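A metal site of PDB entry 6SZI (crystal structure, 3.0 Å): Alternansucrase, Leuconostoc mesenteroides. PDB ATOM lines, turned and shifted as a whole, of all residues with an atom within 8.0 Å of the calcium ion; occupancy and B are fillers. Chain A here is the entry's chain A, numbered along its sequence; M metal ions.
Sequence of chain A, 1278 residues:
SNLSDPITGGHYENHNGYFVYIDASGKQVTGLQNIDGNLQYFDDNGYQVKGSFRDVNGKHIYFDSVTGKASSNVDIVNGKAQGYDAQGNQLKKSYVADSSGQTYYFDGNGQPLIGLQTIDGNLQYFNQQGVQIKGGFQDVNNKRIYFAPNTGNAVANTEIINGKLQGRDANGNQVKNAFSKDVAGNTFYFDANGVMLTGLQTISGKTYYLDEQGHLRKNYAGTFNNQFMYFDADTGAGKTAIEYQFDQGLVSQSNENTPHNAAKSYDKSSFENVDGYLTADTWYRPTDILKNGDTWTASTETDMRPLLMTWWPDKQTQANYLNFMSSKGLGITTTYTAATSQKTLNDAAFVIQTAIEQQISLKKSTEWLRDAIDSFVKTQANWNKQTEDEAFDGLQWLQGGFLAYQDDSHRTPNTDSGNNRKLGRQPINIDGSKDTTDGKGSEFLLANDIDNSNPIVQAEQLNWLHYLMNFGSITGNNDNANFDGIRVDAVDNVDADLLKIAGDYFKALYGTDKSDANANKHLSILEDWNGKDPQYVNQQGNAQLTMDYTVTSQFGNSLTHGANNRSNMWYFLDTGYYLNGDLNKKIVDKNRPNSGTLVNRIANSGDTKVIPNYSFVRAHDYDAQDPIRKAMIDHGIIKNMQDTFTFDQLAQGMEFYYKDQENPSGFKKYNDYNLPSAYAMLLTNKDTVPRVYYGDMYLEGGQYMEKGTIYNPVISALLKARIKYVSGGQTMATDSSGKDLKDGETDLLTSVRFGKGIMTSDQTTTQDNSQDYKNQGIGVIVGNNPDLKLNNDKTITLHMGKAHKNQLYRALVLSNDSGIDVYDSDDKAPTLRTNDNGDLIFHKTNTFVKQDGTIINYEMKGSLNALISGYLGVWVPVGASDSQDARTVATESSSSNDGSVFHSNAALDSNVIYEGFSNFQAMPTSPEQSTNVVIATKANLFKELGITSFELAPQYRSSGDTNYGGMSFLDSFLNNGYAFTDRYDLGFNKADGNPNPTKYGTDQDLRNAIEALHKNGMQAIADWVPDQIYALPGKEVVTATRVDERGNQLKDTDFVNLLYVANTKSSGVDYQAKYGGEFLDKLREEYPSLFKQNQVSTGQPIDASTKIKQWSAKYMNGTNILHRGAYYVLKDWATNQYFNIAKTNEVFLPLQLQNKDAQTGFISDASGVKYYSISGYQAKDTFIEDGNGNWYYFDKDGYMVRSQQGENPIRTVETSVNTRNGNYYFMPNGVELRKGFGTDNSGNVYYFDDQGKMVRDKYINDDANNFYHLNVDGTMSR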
ATOM      1  N   LYS A 422       0.734 -15.317  -6.543  1.00  0.00           N
ATOM      2  CA  LYS A 422       1.588 -15.677  -7.684  1.00  0.00           C
ATOM      3  C   LYS A 422       1.167 -17.059  -8.197  1.00  0.00           C
ATOM      4  O   LYS A 422       1.223 -18.069  -7.466  1.00  0.00           O
ATOM      5  CB  LYS A 422       3.036 -15.687  -7.279  1.00  0.00           C
ATOM      6  CG  LYS A 422       3.552 -14.358  -6.765  1.00  0.00           C
ATOM      7  CD  LYS A 422       4.696 -14.564  -5.805  1.00  0.00           C
ATOM      8  CE  LYS A 422       4.705 -13.529  -4.699  1.00  0.00           C
ATOM      9  NZ  LYS A 422       5.657 -12.456  -5.059  1.00  0.00           N
ATOM     10  N   LEU A 423       0.733 -17.108  -9.454  1.00  0.00           N
ATOM     11  CA  LEU A 423       0.187 -18.343  -9.996  1.00  0.00           C
ATOM     12  C   LEU A 423       1.194 -19.137 -10.800  1.00  0.00           C
ATOM     13  O   LEU A 423       2.039 -18.539 -11.458  1.00  0.00           O
ATOM     14  CB  LEU A 423      -1.002 -18.032 -10.865  1.00  0.00           C
ATOM     15  CG  LEU A 423      -2.095 -17.205 -10.187  1.00  0.00           C
ATOM     16  CD1 LEU A 423      -3.264 -17.120 -11.144  1.00  0.00           C
ATOM     17  CD2 LEU A 423      -2.545 -17.833  -8.882  1.00  0.00           C
ATOM     18  N   GLY A 424       1.163 -20.454 -10.678  1.00  0.00           N
ATOM     19  CA  GLY A 424       1.960 -21.329 -11.561  1.00  0.00           C
ATOM     20  C   GLY A 424       3.439 -21.310 -11.278  1.00  0.00           C
ATOM     21  O   GLY A 424       4.248 -21.441 -12.199  1.00  0.00           O
ATOM     22  N   ARG A 425       3.821 -21.176 -10.015  1.00  0.00           N
ATOM     23  CA  ARG A 425       5.243 -21.185  -9.680  1.00  0.00           C
ATOM     24  C   ARG A 425       5.769 -22.602  -9.465  1.00  0.00           C
ATOM     25  O   ARG A 425       6.394 -22.913  -8.472  1.00  0.00           O
ATOM     26  CB  ARG A 425       5.515 -20.323  -8.447  1.00  0.00           C
ATOM     27  CG  ARG A 425       5.259 -18.850  -8.695  1.00  0.00           C
ATOM     28  CD  ARG A 425       6.069 -18.253  -9.857  1.00  0.00           C
ATOM     29  NE  ARG A 425       5.874 -16.801  -9.865  1.00  0.00           N
ATOM     30  CZ  ARG A 425       6.596 -15.933  -9.173  1.00  0.00           C
ATOM     31  NH1 ARG A 425       7.647 -16.302  -8.441  1.00  0.00           N
ATOM     32  NH2 ARG A 425       6.290 -14.661  -9.230  1.00  0.00           N
ATOM     33  N   GLY A 441       3.118 -22.836 -14.656  1.00  0.00           N
ATOM     34  CA  GLY A 441       2.479 -23.981 -14.062  1.00  0.00           C
ATOM     35  C   GLY A 441       0.977 -23.911 -14.103  1.00  0.00           C
ATOM     36  O   GLY A 441       0.416 -22.845 -13.982  1.00  0.00           O
ATOM     37  N   SER A 442       0.338 -25.068 -14.293  1.00  0.00           N
ATOM     38  CA  SER A 442      -1.097 -25.193 -14.158  1.00  0.00           C
ATOM     39  C   SER A 442      -1.508 -25.125 -12.690  1.00  0.00           C
ATOM     40  O   SER A 442      -1.686 -26.149 -12.076  1.00  0.00           O
ATOM     41  CB  SER A 442      -1.556 -26.533 -14.763  1.00  0.00           C
ATOM     42  OG  SER A 442      -0.971 -26.706 -16.039  1.00  0.00           O
ATOM     43  N   GLU A 443      -1.651 -23.915 -12.147  1.00  0.00           N
ATOM     44  CA  GLU A 443      -1.904 -23.725 -10.703  1.00  0.00           C
ATOM     45  C   GLU A 443      -3.246 -24.270 -10.249  1.00  0.00           C
ATOM     46  O   GLU A 443      -3.406 -24.664  -9.083  1.00  0.00           O
ATOM     47  CB  GLU A 443      -1.817 -22.241 -10.352  1.00  0.00           C
ATOM     48  CG  GLU A 443      -2.010 -21.848  -8.891  1.00  0.00           C
ATOM     49  CD  GLU A 443      -0.944 -22.378  -7.941  1.00  0.00           C
ATOM     50  OE1 GLU A 443       0.220 -21.877  -8.000  1.00  0.00           O
ATOM     51  OE2 GLU A 443      -1.304 -23.251  -7.094  1.00  0.00           O
ATOM     52  N   PHE A 444      -4.184 -24.313 -11.179  1.00  0.00           N
ATOM     53  CA  PHE A 444      -5.550 -24.708 -10.875  1.00  0.00           C
ATOM     54  C   PHE A 444      -5.787 -26.117 -11.288  1.00  0.00           C
ATOM     55  O   PHE A 444      -5.528 -26.465 -12.424  1.00  0.00           O
ATOM     56  CB  PHE A 444      -6.569 -23.808 -11.563  1.00  0.00           C
ATOM     57  CG  PHE A 444      -6.499 -22.383 -11.113  1.00  0.00           C
ATOM     58  CD1 PHE A 444      -7.208 -21.973  -9.995  1.00  0.00           C
ATOM     59  CD2 PHE A 444      -5.704 -21.473 -11.767  1.00  0.00           C
ATOM     60  CE1 PHE A 444      -7.118 -20.673  -9.556  1.00  0.00           C
ATOM     61  CE2 PHE A 444      -5.618 -20.169 -11.341  1.00  0.00           C
ATOM     62  CZ  PHE A 444      -6.330 -19.776 -10.237  1.00  0.00           C
ATOM     63  N   LEU A 445      -6.272 -26.913 -10.338  1.00  0.00           N
ATOM     64  CA  LEU A 445      -6.516 -28.298 -10.553  1.00  0.00           C
ATOM     65  C   LEU A 445      -7.905 -28.656 -10.119  1.00  0.00           C
ATOM     66  O   LEU A 445      -8.715 -29.079 -10.952  1.00  0.00           O
ATOM     67  CB  LEU A 445      -5.481 -29.146  -9.796  1.00  0.00           C
ATOM     68  CG  LEU A 445      -5.636 -30.668  -9.852  1.00  0.00           C
ATOM     69  CD1 LEU A 445      -5.527 -31.160 -11.294  1.00  0.00           C
ATOM     70  CD2 LEU A 445      -4.545 -31.298  -9.016  1.00  0.00           C
ATOM     71  N   LEU A 446      -8.171 -28.539  -8.823  1.00  0.00           N
ATOM     72  CA  LEU A 446      -9.482 -28.965  -8.288  1.00  0.00           C
ATOM     73  C   LEU A 446      -9.915 -28.064  -7.158  1.00  0.00           C
ATOM     74  O   LEU A 446      -9.073 -27.436  -6.486  1.00  0.00           O
ATOM     75  CB  LEU A 446      -9.447 -30.413  -7.804  1.00  0.00           C
ATOM     76  CG  LEU A 446      -9.357 -31.525  -8.881  1.00  0.00           C
ATOM     77  CD1 LEU A 446      -8.886 -32.841  -8.318  1.00  0.00           C
ATOM     78  CD2 LEU A 446     -10.677 -31.777  -9.582  1.00  0.00           C
ATOM     79  N   ASN A 448     -11.098 -25.586  -4.357  1.00  0.00           N
ATOM     80  CA  ASN A 448     -10.573 -24.294  -4.007  1.00  0.00           C
ATOM     81  C   ASN A 448      -9.079 -24.386  -3.973  1.00  0.00           C
ATOM     82  O   ASN A 448      -8.568 -25.129  -3.174  1.00  0.00           O
ATOM     83  CB  ASN A 448     -11.039 -23.867  -2.619  1.00  0.00           C
ATOM     84  CG  ASN A 448     -12.527 -23.660  -2.551  1.00  0.00           C
ATOM     85  OD1 ASN A 448     -13.032 -22.624  -3.042  1.00  0.00           O
ATOM     86  ND2 ASN A 448     -13.240 -24.619  -1.915  1.00  0.00           N
ATOM     87  N   ASP A 449      -8.382 -23.652  -4.826  1.00  0.00           N
ATOM     88  CA  ASP A 449      -6.945 -23.788  -4.908  1.00  0.00           C
ATOM     89  C   ASP A 449      -6.376 -22.807  -3.881  1.00  0.00           C
ATOM     90  O   ASP A 449      -6.662 -21.615  -3.896  1.00  0.00           O
ATOM     91  CB  ASP A 449      -6.443 -23.595  -6.370  1.00  0.00           C
ATOM     92  CG  ASP A 449      -4.936 -23.563  -6.504  1.00  0.00           C
ATOM     93  OD1 ASP A 449      -4.307 -24.632  -6.677  1.00  0.00           O
ATOM     94  OD2 ASP A 449      -4.347 -22.454  -6.442  1.00  0.00           O
ATOM     95  N   ILE A 450      -5.587 -23.334  -2.959  1.00  0.00           N
ATOM     96  CA  ILE A 450      -4.929 -22.586  -1.887  1.00  0.00           C
ATOM     97  C   ILE A 450      -3.748 -21.790  -2.421  1.00  0.00           C
ATOM     98  O   ILE A 450      -2.962 -22.314  -3.212  1.00  0.00           O
ATOM     99  CB  ILE A 450      -4.445 -23.576  -0.804  1.00  0.00           C
ATOM    100  CG1 ILE A 450      -5.660 -24.107  -0.047  1.00  0.00           C
ATOM    101  CG2 ILE A 450      -3.457 -22.943   0.178  1.00  0.00           C
ATOM    102  CD1 ILE A 450      -5.411 -25.428   0.641  1.00  0.00           C
ATOM    103  N   ASP A 451      -3.608 -20.540  -1.968  1.00  0.00           N
ATOM    104  CA  ASP A 451      -2.503 -19.654  -2.346  1.00  0.00           C
ATOM    105  C   ASP A 451      -1.219 -19.954  -1.570  1.00  0.00           C
ATOM    106  O   ASP A 451      -0.882 -19.279  -0.588  1.00  0.00           O
ATOM    107  CB  ASP A 451      -2.874 -18.181  -2.133  1.00  0.00           C
ATOM    108  CG  ASP A 451      -1.761 -17.217  -2.579  1.00  0.00           C
ATOM    109  OD1 ASP A 451      -0.824 -17.641  -3.345  1.00  0.00           O
ATOM    110  OD2 ASP A 451      -1.838 -16.050  -2.101  1.00  0.00           O
ATOM    111  N   ASN A 452      -0.468 -20.944  -2.045  1.00  0.00           N
ATOM    112  CA  ASN A 452       0.802 -21.322  -1.434  1.00  0.00           C
ATOM    113  C   ASN A 452       1.960 -20.400  -1.783  1.00  0.00           C
ATOM    114  O   ASN A 452       3.079 -20.733  -1.494  1.00  0.00           O
ATOM    115  CB  ASN A 452       1.161 -22.760  -1.835  1.00  0.00           C
ATOM    116  CG  ASN A 452       0.145 -23.790  -1.355  1.00  0.00           C
ATOM    117  OD1 ASN A 452      -0.251 -23.802  -0.208  1.00  0.00           O
ATOM    118  ND2 ASN A 452      -0.291 -24.669  -2.274  1.00  0.00           N
ATOM    119  N   ALA A 490       0.643 -33.315  -6.201  1.00  0.00           N
ATOM    120  CA  ALA A 490       0.369 -32.237  -7.149  1.00  0.00           C
ATOM    121  C   ALA A 490       1.441 -31.134  -7.119  1.00  0.00           C
ATOM    122  O   ALA A 490       1.157 -29.959  -6.968  1.00  0.00           O
ATOM    123  CB  ALA A 490      -1.012 -31.639  -6.876  1.00  0.00           C
ATOM    124  N   VAL A 491       2.684 -31.566  -7.268  1.00  0.00           N
ATOM    125  CA  VAL A 491       3.815 -30.679  -7.201  1.00  0.00           C
ATOM    126  C   VAL A 491       3.758 -29.534  -8.210  1.00  0.00           C
ATOM    127  O   VAL A 491       4.138 -28.382  -7.893  1.00  0.00           O
ATOM    128  CB  VAL A 491       5.098 -31.489  -7.413  1.00  0.00           C
ATOM    129  CG1 VAL A 491       6.324 -30.594  -7.683  1.00  0.00           C
ATOM    130  CG2 VAL A 491       5.350 -32.358  -6.188  1.00  0.00           C
ATOM    131  N   ASP A 492       3.335 -29.856  -9.430  1.00  0.00           N
ATOM    132  CA  ASP A 492       3.363 -28.879 -10.517  1.00  0.00           C
ATOM    133  C   ASP A 492       2.185 -27.895 -10.451  1.00  0.00           C
ATOM    134  O   ASP A 492       2.203 -26.850 -11.113  1.00  0.00           O
ATOM    135  CB  ASP A 492       3.435 -29.602 -11.845  1.00  0.00           C
ATOM    136  CG  ASP A 492       4.708 -30.458 -11.985  1.00  0.00           C
ATOM    137  OD1 ASP A 492       5.719 -30.142 -11.319  1.00  0.00           O
ATOM    138  OD2 ASP A 492       4.715 -31.405 -12.799  1.00  0.00           O
ATOM    139  N   ASN A 493       1.216 -28.194  -9.579  1.00  0.00           N
ATOM    140  CA  ASN A 493       0.061 -27.325  -9.343  1.00  0.00           C
ATOM    141  C   ASN A 493       0.113 -26.394  -8.100  1.00  0.00           C
ATOM    142  O   ASN A 493      -0.935 -25.839  -7.697  1.00  0.00           O
ATOM    143  CB  ASN A 493      -1.175 -28.204  -9.190  1.00  0.00           C
ATOM    144  CG  ASN A 493      -1.160 -29.345 -10.146  1.00  0.00           C
ATOM    145  OD1 ASN A 493      -0.513 -30.358  -9.898  1.00  0.00           O
ATOM    146  ND2 ASN A 493      -1.854 -29.194 -11.256  1.00  0.00           N
ATOM    147  N   VAL A 494       1.312 -26.244  -7.525  1.00  0.00           N
ATOM    148  CA  VAL A 494       1.559 -25.426  -6.364  1.00  0.00           C
ATOM    149  C   VAL A 494       2.897 -24.698  -6.492  1.00  0.00           C
ATOM    150  O   VAL A 494       3.671 -24.906  -7.415  1.00  0.00           O
ATOM    151  CB  VAL A 494       1.570 -26.224  -5.020  1.00  0.00           C
ATOM    152  CG1 VAL A 494       0.290 -27.028  -4.834  1.00  0.00           C
ATOM    153  CG2 VAL A 494       2.782 -27.129  -4.935  1.00  0.00           C
ATOM    154  N   ASP A 495       3.116 -23.782  -5.568  1.00  0.00           N
ATOM    155  CA  ASP A 495       4.333 -22.992  -5.507  1.00  0.00           C
ATOM    156  C   ASP A 495       5.440 -23.901  -5.049  1.00  0.00           C
ATOM    157  O   ASP A 495       5.349 -24.543  -3.993  1.00  0.00           O
ATOM    158  CB  ASP A 495       4.142 -21.804  -4.513  1.00  0.00           C
ATOM    159  CG  ASP A 495       5.240 -20.767  -4.600  1.00  0.00           C
ATOM    160  OD1 ASP A 495       6.428 -21.139  -4.587  1.00  0.00           O
ATOM    161  OD2 ASP A 495       4.942 -19.570  -4.633  1.00  0.00           O
ATOM    162  N   PRO A1026      -1.263 -30.111  -0.153  1.00  0.00           N
ATOM    163  CA  PRO A1026      -1.371 -28.698   0.057  1.00  0.00           C
ATOM    164  C   PRO A1026      -2.140 -27.891  -1.026  1.00  0.00           C
ATOM    165  O   PRO A1026      -2.442 -26.713  -0.791  1.00  0.00           O
ATOM    166  CB  PRO A1026       0.098 -28.268   0.094  1.00  0.00           C
ATOM    167  CG  PRO A1026       0.766 -29.178  -0.866  1.00  0.00           C
ATOM    168  CD  PRO A1026       0.031 -30.485  -0.755  1.00  0.00           C
ATOM    169  N   ASP A1027      -2.439 -28.490  -2.179  1.00  0.00           N
ATOM    170  CA  ASP A1027      -2.949 -27.711  -3.315  1.00  0.00           C
ATOM    171  C   ASP A1027      -4.371 -27.192  -3.146  1.00  0.00           C
ATOM    172  O   ASP A1027      -4.656 -26.056  -3.516  1.00  0.00           O
ATOM    173  CB  ASP A1027      -2.879 -28.478  -4.620  1.00  0.00           C
ATOM    174  CG  ASP A1027      -3.409 -27.689  -5.763  1.00  0.00           C
ATOM    175  OD1 ASP A1027      -2.873 -26.591  -6.064  1.00  0.00           O
ATOM    176  OD2 ASP A1027      -4.390 -28.159  -6.345  1.00  0.00           O
ATOM    177  N   GLN A1028      -5.255 -28.003  -2.593  1.00  0.00           N
ATOM    178  CA  GLN A1028      -6.636 -27.572  -2.452  1.00  0.00           C
ATOM    179  C   GLN A1028      -7.377 -28.099  -1.229  1.00  0.00           C
ATOM    180  O   GLN A1028      -6.906 -28.966  -0.480  1.00  0.00           O
ATOM    181  CB  GLN A1028      -7.418 -27.929  -3.721  1.00  0.00           C
ATOM    182  CG  GLN A1028      -7.810 -29.394  -3.852  1.00  0.00           C
ATOM    183  CD  GLN A1028      -6.636 -30.271  -4.135  1.00  0.00           C
ATOM    184  OE1 GLN A1028      -5.802 -29.916  -4.963  1.00  0.00           O
ATOM    185  NE2 GLN A1028      -6.538 -31.414  -3.433  1.00  0.00           N
ATOM    186  N   GLU A1045      -6.310 -23.547 -16.711  1.00  0.00           N
ATOM    187  CA  GLU A1045      -5.514 -24.153 -15.633  1.00  0.00           C
ATOM    188  C   GLU A1045      -4.302 -23.339 -15.172  1.00  0.00           C
ATOM    189  O   GLU A1045      -3.940 -23.405 -14.006  1.00  0.00           O
ATOM    190  CB  GLU A1045      -5.061 -25.554 -16.032  1.00  0.00           C
ATOM    191  CG  GLU A1045      -4.027 -25.622 -17.157  1.00  0.00           C
ATOM    192  CD  GLU A1045      -3.902 -27.019 -17.748  1.00  0.00           C
ATOM    193  OE1 GLU A1045      -4.875 -27.506 -18.362  1.00  0.00           O
ATOM    194  OE2 GLU A1045      -2.856 -27.655 -17.587  1.00  0.00           O
ATOM    195  N   ASN A1117      -6.323 -18.889  -4.350  1.00  0.00           N
ATOM    196  CA  ASN A1117      -6.079 -18.388  -5.704  1.00  0.00           C
ATOM    197  C   ASN A1117      -7.341 -18.382  -6.515  1.00  0.00           C
ATOM    198  O   ASN A1117      -7.482 -17.549  -7.411  1.00  0.00           O
ATOM    199  CB  ASN A1117      -5.056 -19.250  -6.421  1.00  0.00           C
ATOM    200  CG  ASN A1117      -3.673 -19.089  -5.857  1.00  0.00           C
ATOM    201  OD1 ASN A1117      -3.324 -18.025  -5.360  1.00  0.00           O
ATOM    202  ND2 ASN A1117      -2.866 -20.130  -5.954  1.00  0.00           N
ATOM    203  N   GLY A1118      -8.224 -19.326  -6.246  1.00  0.00           N
ATOM    204  CA  GLY A1118      -9.470 -19.389  -6.970  1.00  0.00           C
ATOM    205  C   GLY A1118     -10.333 -20.590  -6.620  1.00  0.00           C
ATOM    206  O   GLY A1118     -10.249 -21.145  -5.521  1.00  0.00           O
HETATM  207 CA    CA M   1      -2.578 -24.598  -7.030  1.00  0.00          CA
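The calcium ion is bound by the side-chain carboxylate (OD1) of Asp 449, the side-chain carboxylate (OE2) of Glu 443, the backbone carbonyl oxygen (O) of Asn 493, the backbone carbonyl oxygen (O) of Glu 443, the side-chain carboxylate (OD1) of Asp 1027 and the side-chain carboxylate (OD2) of Asp 449.
N of Asn 1117 sits at hydrogen-bond distance from O of Asp 449, at 2.8 Å.
O of Gly 1118 lies within hydrogen-bond range of N of Asp 449, at 3.2 Å.
The side-chain carboxylate (OE1) of Glu 443 sits at hydrogen-bond distance from the backbone NH (N) of Gly 424, 3.2 Å away.
The backbone NH (N) of Glu 443 lies within hydrogen-bond range of the backbone carbonyl oxygen (O) of Glu 1045 (3.0 Å).
ND2 of Asn 493 is in hydrogen-bond range of O of Ser 442 (3.2 Å).
The side-chain amide oxygen (OD1) of Asn 493 sits close to the backbone carbonyl oxygen (O) of Ala 490.
O of Asp 1027 sits at hydrogen-bond distance from N of Ile 450, 2.9 Å away.
The side-chain amide oxygen of Gln 1028 sits close to the side-chain carboxylate of Asp 1027 (2.6 Å).
Of the 27 residues printed, 4 come within 4 Å of the calcium ion.
Along chain A the residues within 4 Å of the calcium ion span positions 443 to 1027.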
